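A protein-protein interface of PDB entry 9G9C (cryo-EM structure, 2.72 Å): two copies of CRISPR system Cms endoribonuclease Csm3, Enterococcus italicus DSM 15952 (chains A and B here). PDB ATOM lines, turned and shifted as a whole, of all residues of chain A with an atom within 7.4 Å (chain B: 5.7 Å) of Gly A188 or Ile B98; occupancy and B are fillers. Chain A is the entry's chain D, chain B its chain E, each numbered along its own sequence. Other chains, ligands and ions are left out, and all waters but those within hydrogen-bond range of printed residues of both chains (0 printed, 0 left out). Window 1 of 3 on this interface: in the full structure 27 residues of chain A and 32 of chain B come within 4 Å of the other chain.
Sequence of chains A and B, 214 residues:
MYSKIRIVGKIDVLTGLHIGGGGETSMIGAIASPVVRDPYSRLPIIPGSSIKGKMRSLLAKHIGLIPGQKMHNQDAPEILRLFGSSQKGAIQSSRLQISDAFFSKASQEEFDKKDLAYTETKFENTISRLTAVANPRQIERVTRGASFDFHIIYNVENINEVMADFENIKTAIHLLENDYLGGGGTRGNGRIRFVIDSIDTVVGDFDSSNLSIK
The side-chain hydroxyl of Thr A186 lies within hydrogen-bond range of the side-chain amino group of Lys B52, at 2.7 Å. The backbone NH of Gly A188 is in hydrogen-bond range of the backbone carbonyl oxygen of Ile B98, 2.7 Å away. The side-chain carboxylate of Asp B100 is in salt-bridge range of the guanidinium group of Arg A141, 3.1 Å away. The backbone carbonyl oxygen (O) of Thr A186 lies within hydrogen-bond range of the backbone NH (N) of Ile B98, 3.2 Å away. OG of Ser B99 is in hydrogen-bond range of NH1 of Arg A191 (3.0 Å). The backbone NH of Ser B49 is in hydrogen-bond range of the backbone carbonyl oxygen of Arg A187 (2.8 Å). The backbone carbonyl oxygen of Gly A188 sits close to the side-chain carboxylate of Asp B100, at 3.1 Å. NZ of Lys A122 is in hydrogen-bond range of OG of Ser B49 (2.9 Å).
The side-chain carboxylate (OD1) of Asp B100 sits at hydrogen-bond distance from the backbone NH (N) of Gly B48 (2.7 Å). OG1 of Thr A15 sits at hydrogen-bond distance from N of Gly A190. The backbone NH (N) of Ser B99 is in hydrogen-bond range of the backbone carbonyl oxygen (O) of His B151 (3.0 Å). N of Leu A14 is in hydrogen-bond range of O of Arg A191, 2.7 Å away. The side-chain amide oxygen (OD1) of Asn A189 lies within hydrogen-bond range of the guanidinium group (NH1) of Arg A141, 2.6 Å away. The side-chain amino group of Lys B52 sits at hydrogen-bond distance from the backbone carbonyl oxygen of Phe B83 (3.1 Å).
Among the printed residues, merely in contact across the chains: Thr A15 with Ser B99 (3.3 Å), Tyr A180 with Gln B97 (3.2 Å), Thr A186 with Leu B96 (3.8 Å), Thr A186 with Gln B97 (3.8 Å), Arg A187 with Gly B48 (3.2 Å), Arg A187 with Lys B52 (3.6 Å), Arg A187 with Ile B98 (3.2 Å), Arg A187 with Asp B100 (3.9 Å), Gly A188 with Ser B99 (3.6 Å) and Arg A191 with His B151 (3.5 Å).
Gly A16 touches none of the printed residues of chain B. Of the printed residues of chain B, Arg A141 touches Asp B100 (3.1 Å). Gly A185 touches none of the printed residues of chain B. Gly A188 touches just these residues of chain B: Ile B98 (2.7 Å), Ser B99 (3.6 Å) and Asp B100 (3.1 Å). Printed residues of chain B within 4 Å of Arg A191: Ser B99 (3.0 Å) and His B151 (3.5 Å). Of the printed residues of chain A, Gly B48 touches Arg A187. Printed residues of chain A within 4 Å of Ser B49: Lys A122 and Arg A187. Of chain A, only Thr A186 (3.2 Å), Arg A187 (3.2 Å) and Gly A188 (2.7 Å) come within 4 Å of Ile B98. Printed residues of chain A within 4 Å of Asp B100: Arg A141 (3.1 Å), Arg A187 (3.9 Å) and Gly A188 (3.1 Å). The nearest printed residue of chain B that does not touch Arg A187 is Ser B99 (5.3 Å).
Of the 15 printed residues of chain A, 8 touch a printed residue of chain B. Printed residues of chain A that touch a printed residue of chain B: Thr A15, Lys A122, Arg A141, Tyr A180, Thr A186, Arg A187, Gly A188 and Arg A191. Along chain A the printed residues that touch a printed residue of chain B span positions 15 to 191. Of the 14 printed residues of chain B, 9 touch a printed residue of chain A. Printed residues of chain B that touch a printed residue of chain A: Gly B48, Ser B49, Lys B52, Leu B96, Gln B97, Ile B98, Ser B99, Asp B100 and His B151. Among the printed residues, 18 pairs touch across the chains.
No position is printed for both chains.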
ATOM      1  N   LEU A  14       8.229  -7.558 -29.102  1.00  0.00           N
ATOM      2  CA  LEU A  14       8.459  -6.263 -29.732  1.00  0.00           C
ATOM      3  C   LEU A  14       8.749  -5.163 -28.722  1.00  0.00           C
ATOM      4  O   LEU A  14       9.428  -4.189 -29.058  1.00  0.00           O
ATOM      5  CB  LEU A  14       7.258  -5.872 -30.597  1.00  0.00           C
ATOM      6  CG  LEU A  14       6.865  -6.890 -31.671  1.00  0.00           C
ATOM      7  CD1 LEU A  14       5.740  -6.357 -32.540  1.00  0.00           C
ATOM      8  CD2 LEU A  14       8.066  -7.267 -32.519  1.00  0.00           C
ATOM      9  N   THR A  15       8.227  -5.303 -27.506  1.00  0.00           N
ATOM     10  CA  THR A  15       8.592  -4.396 -26.401  1.00  0.00           C
ATOM     11  C   THR A  15       8.827  -5.342 -25.251  1.00  0.00           C
ATOM     12  O   THR A  15       8.327  -6.475 -25.342  1.00  0.00           O
ATOM     13  CB  THR A  15       7.520  -3.357 -26.080  1.00  0.00           C
ATOM     14  OG1 THR A  15       6.351  -4.108 -25.773  1.00  0.00           O
ATOM     15  CG2 THR A  15       7.278  -2.389 -27.225  1.00  0.00           C
ATOM     16  N   GLY A  16       9.462  -4.909 -24.166  1.00  0.00           N
ATOM     17  CA  GLY A  16       9.814  -5.880 -23.113  1.00  0.00           C
ATOM     18  C   GLY A  16       8.575  -6.511 -22.523  1.00  0.00           C
ATOM     19  O   GLY A  16       7.583  -5.788 -22.333  1.00  0.00           O
ATOM     20  N   LEU A  17       8.627  -7.809 -22.222  1.00  0.00           N
ATOM     21  CA  LEU A  17       7.413  -8.516 -21.748  1.00  0.00           C
ATOM     22  C   LEU A  17       7.552  -8.848 -20.261  1.00  0.00           C
ATOM     23  O   LEU A  17       8.540  -9.502 -19.889  1.00  0.00           O
ATOM     24  CB  LEU A  17       7.263  -9.786 -22.579  1.00  0.00           C
ATOM     25  CG  LEU A  17       6.182 -10.770 -22.124  1.00  0.00           C
ATOM     26  CD1 LEU A  17       4.799 -10.173 -22.282  1.00  0.00           C
ATOM     27  CD2 LEU A  17       6.299 -12.072 -22.891  1.00  0.00           C
ATOM     28  N   LYS A 122      14.087  -3.186 -15.515  1.00  0.00           N
ATOM     29  CA  LYS A 122      13.651  -1.842 -15.966  1.00  0.00           C
ATOM     30  C   LYS A 122      13.426  -0.988 -14.714  1.00  0.00           C
ATOM     31  O   LYS A 122      12.740  -1.462 -13.793  1.00  0.00           O
ATOM     32  CB  LYS A 122      12.389  -1.939 -16.831  1.00  0.00           C
ATOM     33  CG  LYS A 122      11.907  -0.641 -17.462  1.00  0.00           C
ATOM     34  CD  LYS A 122      10.546  -0.792 -18.129  1.00  0.00           C
ATOM     35  CE  LYS A 122      10.165   0.380 -18.976  1.00  0.00           C
ATOM     36  NZ  LYS A 122      10.121   1.622 -18.203  1.00  0.00           N
ATOM     37  N   ARG A 141      11.809  -7.475 -17.384  1.00  0.00           N
ATOM     38  CA  ARG A 141      11.083  -7.668 -18.660  1.00  0.00           C
ATOM     39  C   ARG A 141      11.924  -8.584 -19.549  1.00  0.00           C
ATOM     40  O   ARG A 141      13.146  -8.389 -19.587  1.00  0.00           O
ATOM     41  CB  ARG A 141      10.840  -6.332 -19.362  1.00  0.00           C
ATOM     42  CG  ARG A 141       9.932  -5.355 -18.633  1.00  0.00           C
ATOM     43  CD  ARG A 141       9.489  -4.276 -19.599  1.00  0.00           C
ATOM     44  NE  ARG A 141      10.623  -3.711 -20.337  1.00  0.00           N
ATOM     45  CZ  ARG A 141      10.529  -2.785 -21.282  1.00  0.00           C
ATOM     46  NH1 ARG A 141       9.353  -2.478 -21.796  1.00  0.00           N
ATOM     47  NH2 ARG A 141      11.614  -2.176 -21.718  1.00  0.00           N
ATOM     48  N   TYR A 180      -1.180  -6.018 -26.132  1.00  0.00           N
ATOM     49  CA  TYR A 180      -0.030  -6.486 -25.381  1.00  0.00           C
ATOM     50  C   TYR A 180      -0.350  -7.806 -24.696  1.00  0.00           C
ATOM     51  O   TYR A 180      -1.512  -8.152 -24.475  1.00  0.00           O
ATOM     52  CB  TYR A 180       0.405  -5.450 -24.339  1.00  0.00           C
ATOM     53  CG  TYR A 180      -0.695  -5.015 -23.400  1.00  0.00           C
ATOM     54  CD1 TYR A 180      -1.538  -3.964 -23.729  1.00  0.00           C
ATOM     55  CD2 TYR A 180      -0.884  -5.646 -22.179  1.00  0.00           C
ATOM     56  CE1 TYR A 180      -2.540  -3.559 -22.873  1.00  0.00           C
ATOM     57  CE2 TYR A 180      -1.881  -5.246 -21.316  1.00  0.00           C
ATOM     58  CZ  TYR A 180      -2.707  -4.202 -21.668  1.00  0.00           C
ATOM     59  OH  TYR A 180      -3.703  -3.801 -20.810  1.00  0.00           O
ATOM     60  N   GLY A 184       2.275  -4.736 -17.624  1.00  0.00           N
ATOM     61  CA  GLY A 184       1.882  -3.345 -17.734  1.00  0.00           C
ATOM     62  C   GLY A 184       1.991  -2.826 -19.152  1.00  0.00           C
ATOM     63  O   GLY A 184       2.813  -1.952 -19.442  1.00  0.00           O
ATOM     64  N   GLY A 185       1.155  -3.352 -20.043  1.00  0.00           N
ATOM     65  CA  GLY A 185       1.281  -3.085 -21.462  1.00  0.00           C
ATOM     66  C   GLY A 185       0.767  -1.747 -21.930  1.00  0.00           C
ATOM     67  O   GLY A 185       1.081  -1.340 -23.051  1.00  0.00           O
ATOM     68  N   THR A 186      -0.016  -1.051 -21.110  1.00  0.00           N
ATOM     69  CA  THR A 186      -0.439   0.295 -21.461  1.00  0.00           C
ATOM     70  C   THR A 186       0.683   1.310 -21.301  1.00  0.00           C
ATOM     71  O   THR A 186       0.534   2.452 -21.748  1.00  0.00           O
ATOM     72  CB  THR A 186      -1.643   0.706 -20.613  1.00  0.00           C
ATOM     73  OG1 THR A 186      -1.232   0.893 -19.254  1.00  0.00           O
ATOM     74  CG2 THR A 186      -2.695  -0.382 -20.662  1.00  0.00           C
ATOM     75  N   ARG A 187       1.791   0.919 -20.674  1.00  0.00           N
ATOM     76  CA  ARG A 187       2.973   1.759 -20.534  1.00  0.00           C
ATOM     77  C   ARG A 187       4.143   1.254 -21.370  1.00  0.00           C
ATOM     78  O   ARG A 187       5.298   1.550 -21.053  1.00  0.00           O
ATOM     79  CB  ARG A 187       3.377   1.863 -19.063  1.00  0.00           C
ATOM     80  CG  ARG A 187       2.422   2.676 -18.213  1.00  0.00           C
ATOM     81  CD  ARG A 187       2.730   2.524 -16.738  1.00  0.00           C
ATOM     82  NE  ARG A 187       2.632   1.134 -16.306  1.00  0.00           N
ATOM     83  CZ  ARG A 187       1.519   0.566 -15.864  1.00  0.00           C
ATOM     84  NH1 ARG A 187       0.388   1.242 -15.766  1.00  0.00           N
ATOM     85  NH2 ARG A 187       1.543  -0.716 -15.508  1.00  0.00           N
ATOM     86  N   GLY A 188       3.850   0.549 -22.466  1.00  0.00           N
ATOM     87  CA  GLY A 188       4.919   0.161 -23.407  1.00  0.00           C
ATOM     88  C   GLY A 188       5.480  -1.217 -23.177  1.00  0.00           C
ATOM     89  O   GLY A 188       6.676  -1.411 -23.458  1.00  0.00           O
ATOM     90  N   ASN A 189       4.667  -2.150 -22.699  1.00  0.00           N
ATOM     91  CA  ASN A 189       5.244  -3.476 -22.376  1.00  0.00           C
ATOM     92  C   ASN A 189       4.426  -4.589 -23.022  1.00  0.00           C
ATOM     93  O   ASN A 189       3.236  -4.383 -23.263  1.00  0.00           O
ATOM     94  CB  ASN A 189       5.337  -3.700 -20.872  1.00  0.00           C
ATOM     95  CG  ASN A 189       6.035  -2.574 -20.148  1.00  0.00           C
ATOM     96  OD1 ASN A 189       7.163  -2.213 -20.496  1.00  0.00           O
ATOM     97  ND2 ASN A 189       5.383  -1.997 -19.149  1.00  0.00           N
ATOM     98  N   GLY A 190       5.067  -5.685 -23.395  1.00  0.00           N
ATOM     99  CA  GLY A 190       4.348  -6.859 -23.835  1.00  0.00           C
ATOM    100  C   GLY A 190       3.869  -6.863 -25.266  1.00  0.00           C
ATOM    101  O   GLY A 190       3.118  -7.770 -25.639  1.00  0.00           O
ATOM    102  N   ARG A 191       4.259  -5.884 -26.080  1.00  0.00           N
ATOM    103  CA  ARG A 191       3.904  -5.919 -27.493  1.00  0.00           C
ATOM    104  C   ARG A 191       4.560  -7.122 -28.152  1.00  0.00           C
ATOM    105  O   ARG A 191       5.757  -7.363 -27.976  1.00  0.00           O
ATOM    106  CB  ARG A 191       4.338  -4.634 -28.189  1.00  0.00           C
ATOM    107  CG  ARG A 191       3.559  -3.403 -27.775  1.00  0.00           C
ATOM    108  CD  ARG A 191       3.955  -2.224 -28.635  1.00  0.00           C
ATOM    109  NE  ARG A 191       3.800  -2.510 -30.054  1.00  0.00           N
ATOM    110  CZ  ARG A 191       4.399  -1.832 -31.022  1.00  0.00           C
ATOM    111  NH1 ARG A 191       5.211  -0.821 -30.758  1.00  0.00           N
ATOM    112  NH2 ARG A 191       4.183  -2.180 -32.286  1.00  0.00           N
ATOM    113  N   GLY B  48       7.725   3.844 -22.996  1.00  0.00           N
ATOM    114  CA  GLY B  48       6.334   4.250 -23.077  1.00  0.00           C
ATOM    115  C   GLY B  48       5.773   4.671 -21.737  1.00  0.00           C
ATOM    116  O   GLY B  48       4.855   5.493 -21.675  1.00  0.00           O
ATOM    117  N   SER B  49       6.315   4.119 -20.649  1.00  0.00           N
ATOM    118  CA  SER B  49       5.903   4.542 -19.316  1.00  0.00           C
ATOM    119  C   SER B  49       6.276   5.996 -19.061  1.00  0.00           C
ATOM    120  O   SER B  49       5.492   6.743 -18.468  1.00  0.00           O
ATOM    121  CB  SER B  49       6.525   3.628 -18.264  1.00  0.00           C
ATOM    122  OG  SER B  49       7.874   3.339 -18.575  1.00  0.00           O
ATOM    123  N   ILE B  51       6.677   8.449 -21.359  1.00  0.00           N
ATOM    124  CA  ILE B  51       5.799   9.293 -22.166  1.00  0.00           C
ATOM    125  C   ILE B  51       4.405   9.340 -21.559  1.00  0.00           C
ATOM    126  O   ILE B  51       3.803  10.411 -21.424  1.00  0.00           O
ATOM    127  CB  ILE B  51       5.753   8.789 -23.619  1.00  0.00           C
ATOM    128  CG1 ILE B  51       7.156   8.457 -24.122  1.00  0.00           C
ATOM    129  CG2 ILE B  51       5.094   9.820 -24.519  1.00  0.00           C
ATOM    130  CD1 ILE B  51       7.169   7.797 -25.482  1.00  0.00           C
ATOM    131  N   LYS B  52       3.869   8.174 -21.187  1.00  0.00           N
ATOM    132  CA  LYS B  52       2.523   8.123 -20.630  1.00  0.00           C
ATOM    133  C   LYS B  52       2.432   8.902 -19.327  1.00  0.00           C
ATOM    134  O   LYS B  52       1.487   9.671 -19.123  1.00  0.00           O
ATOM    135  CB  LYS B  52       2.093   6.674 -20.413  1.00  0.00           C
ATOM    136  CG  LYS B  52       0.643   6.531 -19.993  1.00  0.00           C
ATOM    137  CD  LYS B  52       0.268   5.082 -19.760  1.00  0.00           C
ATOM    138  CE  LYS B  52      -1.191   4.950 -19.369  1.00  0.00           C
ATOM    139  NZ  LYS B  52      -1.525   3.567 -18.936  1.00  0.00           N
ATOM    140  N   MET B  55       2.756  12.769 -20.088  1.00  0.00           N
ATOM    141  CA  MET B  55       1.530  13.253 -20.712  1.00  0.00           C
ATOM    142  C   MET B  55       0.381  13.304 -19.715  1.00  0.00           C
ATOM    143  O   MET B  55      -0.373  14.284 -19.680  1.00  0.00           O
ATOM    144  CB  MET B  55       1.165  12.355 -21.894  1.00  0.00           C
ATOM    145  CG  MET B  55       2.096  12.471 -23.085  1.00  0.00           C
ATOM    146  SD  MET B  55       1.528  11.526 -24.513  1.00  0.00           S
ATOM    147  CE  MET B  55      -0.136  12.151 -24.707  1.00  0.00           C
ATOM    148  N   PHE B  83      -6.159   7.303 -19.824  1.00  0.00           N
ATOM    149  CA  PHE B  83      -4.948   6.637 -19.369  1.00  0.00           C
ATOM    150  C   PHE B  83      -5.206   5.486 -18.407  1.00  0.00           C
ATOM    151  O   PHE B  83      -4.272   4.739 -18.102  1.00  0.00           O
ATOM    152  CB  PHE B  83      -4.011   7.653 -18.708  1.00  0.00           C
ATOM    153  CG  PHE B  83      -3.536   8.730 -19.639  1.00  0.00           C
ATOM    154  CD1 PHE B  83      -2.500   8.491 -20.524  1.00  0.00           C
ATOM    155  CD2 PHE B  83      -4.129   9.980 -19.631  1.00  0.00           C
ATOM    156  CE1 PHE B  83      -2.065   9.480 -21.381  1.00  0.00           C
ATOM    157  CE2 PHE B  83      -3.698  10.970 -20.486  1.00  0.00           C
ATOM    158  CZ  PHE B  83      -2.664  10.719 -21.362  1.00  0.00           C
ATOM    159  N   LEU B  96      -5.560   4.398 -24.065  1.00  0.00           N
ATOM    160  CA  LEU B  96      -4.244   4.639 -24.643  1.00  0.00           C
ATOM    161  C   LEU B  96      -3.262   3.574 -24.174  1.00  0.00           C
ATOM    162  O   LEU B  96      -3.067   3.390 -22.967  1.00  0.00           O
ATOM    163  CB  LEU B  96      -3.726   6.025 -24.262  1.00  0.00           C
ATOM    164  CG  LEU B  96      -4.237   7.231 -25.045  1.00  0.00           C
ATOM    165  CD1 LEU B  96      -3.515   8.487 -24.593  1.00  0.00           C
ATOM    166  CD2 LEU B  96      -4.063   7.014 -26.535  1.00  0.00           C
ATOM    167  N   GLN B  97      -2.645   2.885 -25.126  1.00  0.00           N
ATOM    168  CA  GLN B  97      -1.505   2.012 -24.876  1.00  0.00           C
ATOM    169  C   GLN B  97      -0.311   2.633 -25.587  1.00  0.00           C
ATOM    170  O   GLN B  97      -0.235   2.611 -26.820  1.00  0.00           O
ATOM    171  CB  GLN B  97      -1.775   0.594 -25.373  1.00  0.00           C
ATOM    172  CG  GLN B  97      -3.054  -0.009 -24.834  1.00  0.00           C
ATOM    173  CD  GLN B  97      -3.350  -1.367 -25.429  1.00  0.00           C
ATOM    174  OE1 GLN B  97      -2.613  -1.856 -26.284  1.00  0.00           O
ATOM    175  NE2 GLN B  97      -4.435  -1.985 -24.981  1.00  0.00           N
ATOM    176  N   ILE B  98       0.607   3.201 -24.811  1.00  0.00           N
ATOM    177  CA  ILE B  98       1.749   3.934 -25.341  1.00  0.00           C
ATOM    178  C   ILE B  98       2.963   3.021 -25.306  1.00  0.00           C
ATOM    179  O   ILE B  98       3.335   2.516 -24.243  1.00  0.00           O
ATOM    180  CB  ILE B  98       2.002   5.221 -24.540  1.00  0.00           C
ATOM    181  CG1 ILE B  98       0.795   6.153 -24.642  1.00  0.00           C
ATOM    182  CG2 ILE B  98       3.261   5.914 -25.031  1.00  0.00           C
ATOM    183  CD1 ILE B  98       0.981   7.471 -23.942  1.00  0.00           C
ATOM    184  N   SER B  99       3.584   2.817 -26.462  1.00  0.00           N
ATOM    185  CA  SER B  99       4.708   1.906 -26.584  1.00  0.00           C
ATOM    186  C   SER B  99       6.031   2.638 -26.382  1.00  0.00           C
ATOM    187  O   SER B  99       6.096   3.867 -26.337  1.00  0.00           O
ATOM    188  CB  SER B  99       4.691   1.220 -27.949  1.00  0.00           C
ATOM    189  OG  SER B  99       5.818   0.381 -28.112  1.00  0.00           O
ATOM    190  N   ASP B 100       7.090   1.839 -26.275  1.00  0.00           N
ATOM    191  CA  ASP B 100       8.451   2.406 -26.138  1.00  0.00           C
ATOM    192  C   ASP B 100       8.875   2.978 -27.487  1.00  0.00           C
ATOM    193  O   ASP B 100       8.695   2.281 -28.495  1.00  0.00           O
ATOM    194  CB  ASP B 100       9.422   1.340 -25.663  1.00  0.00           C
ATOM    195  CG  ASP B 100       9.128   0.750 -24.291  1.00  0.00           C
ATOM    196  OD1 ASP B 100       8.190   1.240 -23.631  1.00  0.00           O
ATOM    197  OD2 ASP B 100       9.830  -0.205 -23.901  1.00  0.00           O
ATOM    198  N   HIS B 151       4.838   4.854 -31.153  1.00  0.00           N
ATOM    199  CA  HIS B 151       3.716   4.008 -31.542  1.00  0.00           C
ATOM    200  C   HIS B 151       2.711   4.006 -30.400  1.00  0.00           C
ATOM    201  O   HIS B 151       3.064   3.668 -29.266  1.00  0.00           O
ATOM    202  CB  HIS B 151       4.202   2.587 -31.851  1.00  0.00           C
ATOM    203  CG  HIS B 151       3.107   1.613 -32.157  1.00  0.00           C
ATOM    204  ND1 HIS B 151       2.258   1.117 -31.191  1.00  0.00           N
ATOM    205  CD2 HIS B 151       2.740   1.023 -33.319  1.00  0.00           C
ATOM    206  CE1 HIS B 151       1.407   0.274 -31.749  1.00  0.00           C
ATOM    207  NE2 HIS B 151       1.679   0.199 -33.037  1.00  0.00           N
ATOM    208  N   ILE B 152       1.471   4.391 -30.691  1.00  0.00           N
ATOM    209  CA  ILE B 152       0.411   4.483 -29.694  1.00  0.00           C
ATOM    210  C   ILE B 152      -0.824   3.781 -30.240  1.00  0.00           C
ATOM    211  O   ILE B 152      -1.095   3.835 -31.443  1.00  0.00           O
ATOM    212  CB  ILE B 152       0.097   5.955 -29.341  1.00  0.00           C
ATOM    213  CG1 ILE B 152       1.336   6.647 -28.773  1.00  0.00           C
ATOM    214  CG2 ILE B 152      -1.043   6.046 -28.347  1.00  0.00           C
ATOM    215  CD1 ILE B 152       1.097   8.084 -28.371  1.00  0.00           C
ATOM    216  N   ILE B 153      -1.563   3.106 -29.363  1.00  0.00           N
ATOM    217  CA  ILE B 153      -2.817   2.456 -29.725  1.00  0.00           C
ATOM    218  C   ILE B 153      -3.943   3.102 -28.930  1.00  0.00           C
ATOM    219  O   ILE B 153      -3.825   3.282 -27.714  1.00  0.00           O
ATOM    220  CB  ILE B 153      -2.768   0.940 -29.470  1.00  0.00           C
ATOM    221  CG1 ILE B 153      -1.726   0.284 -30.372  1.00  0.00           C
ATOM    222  CG2 ILE B 153      -4.130   0.316 -29.705  1.00  0.00           C
ATOM    223  CD1 ILE B 153      -2.072   0.346 -31.838  1.00  0.00           C
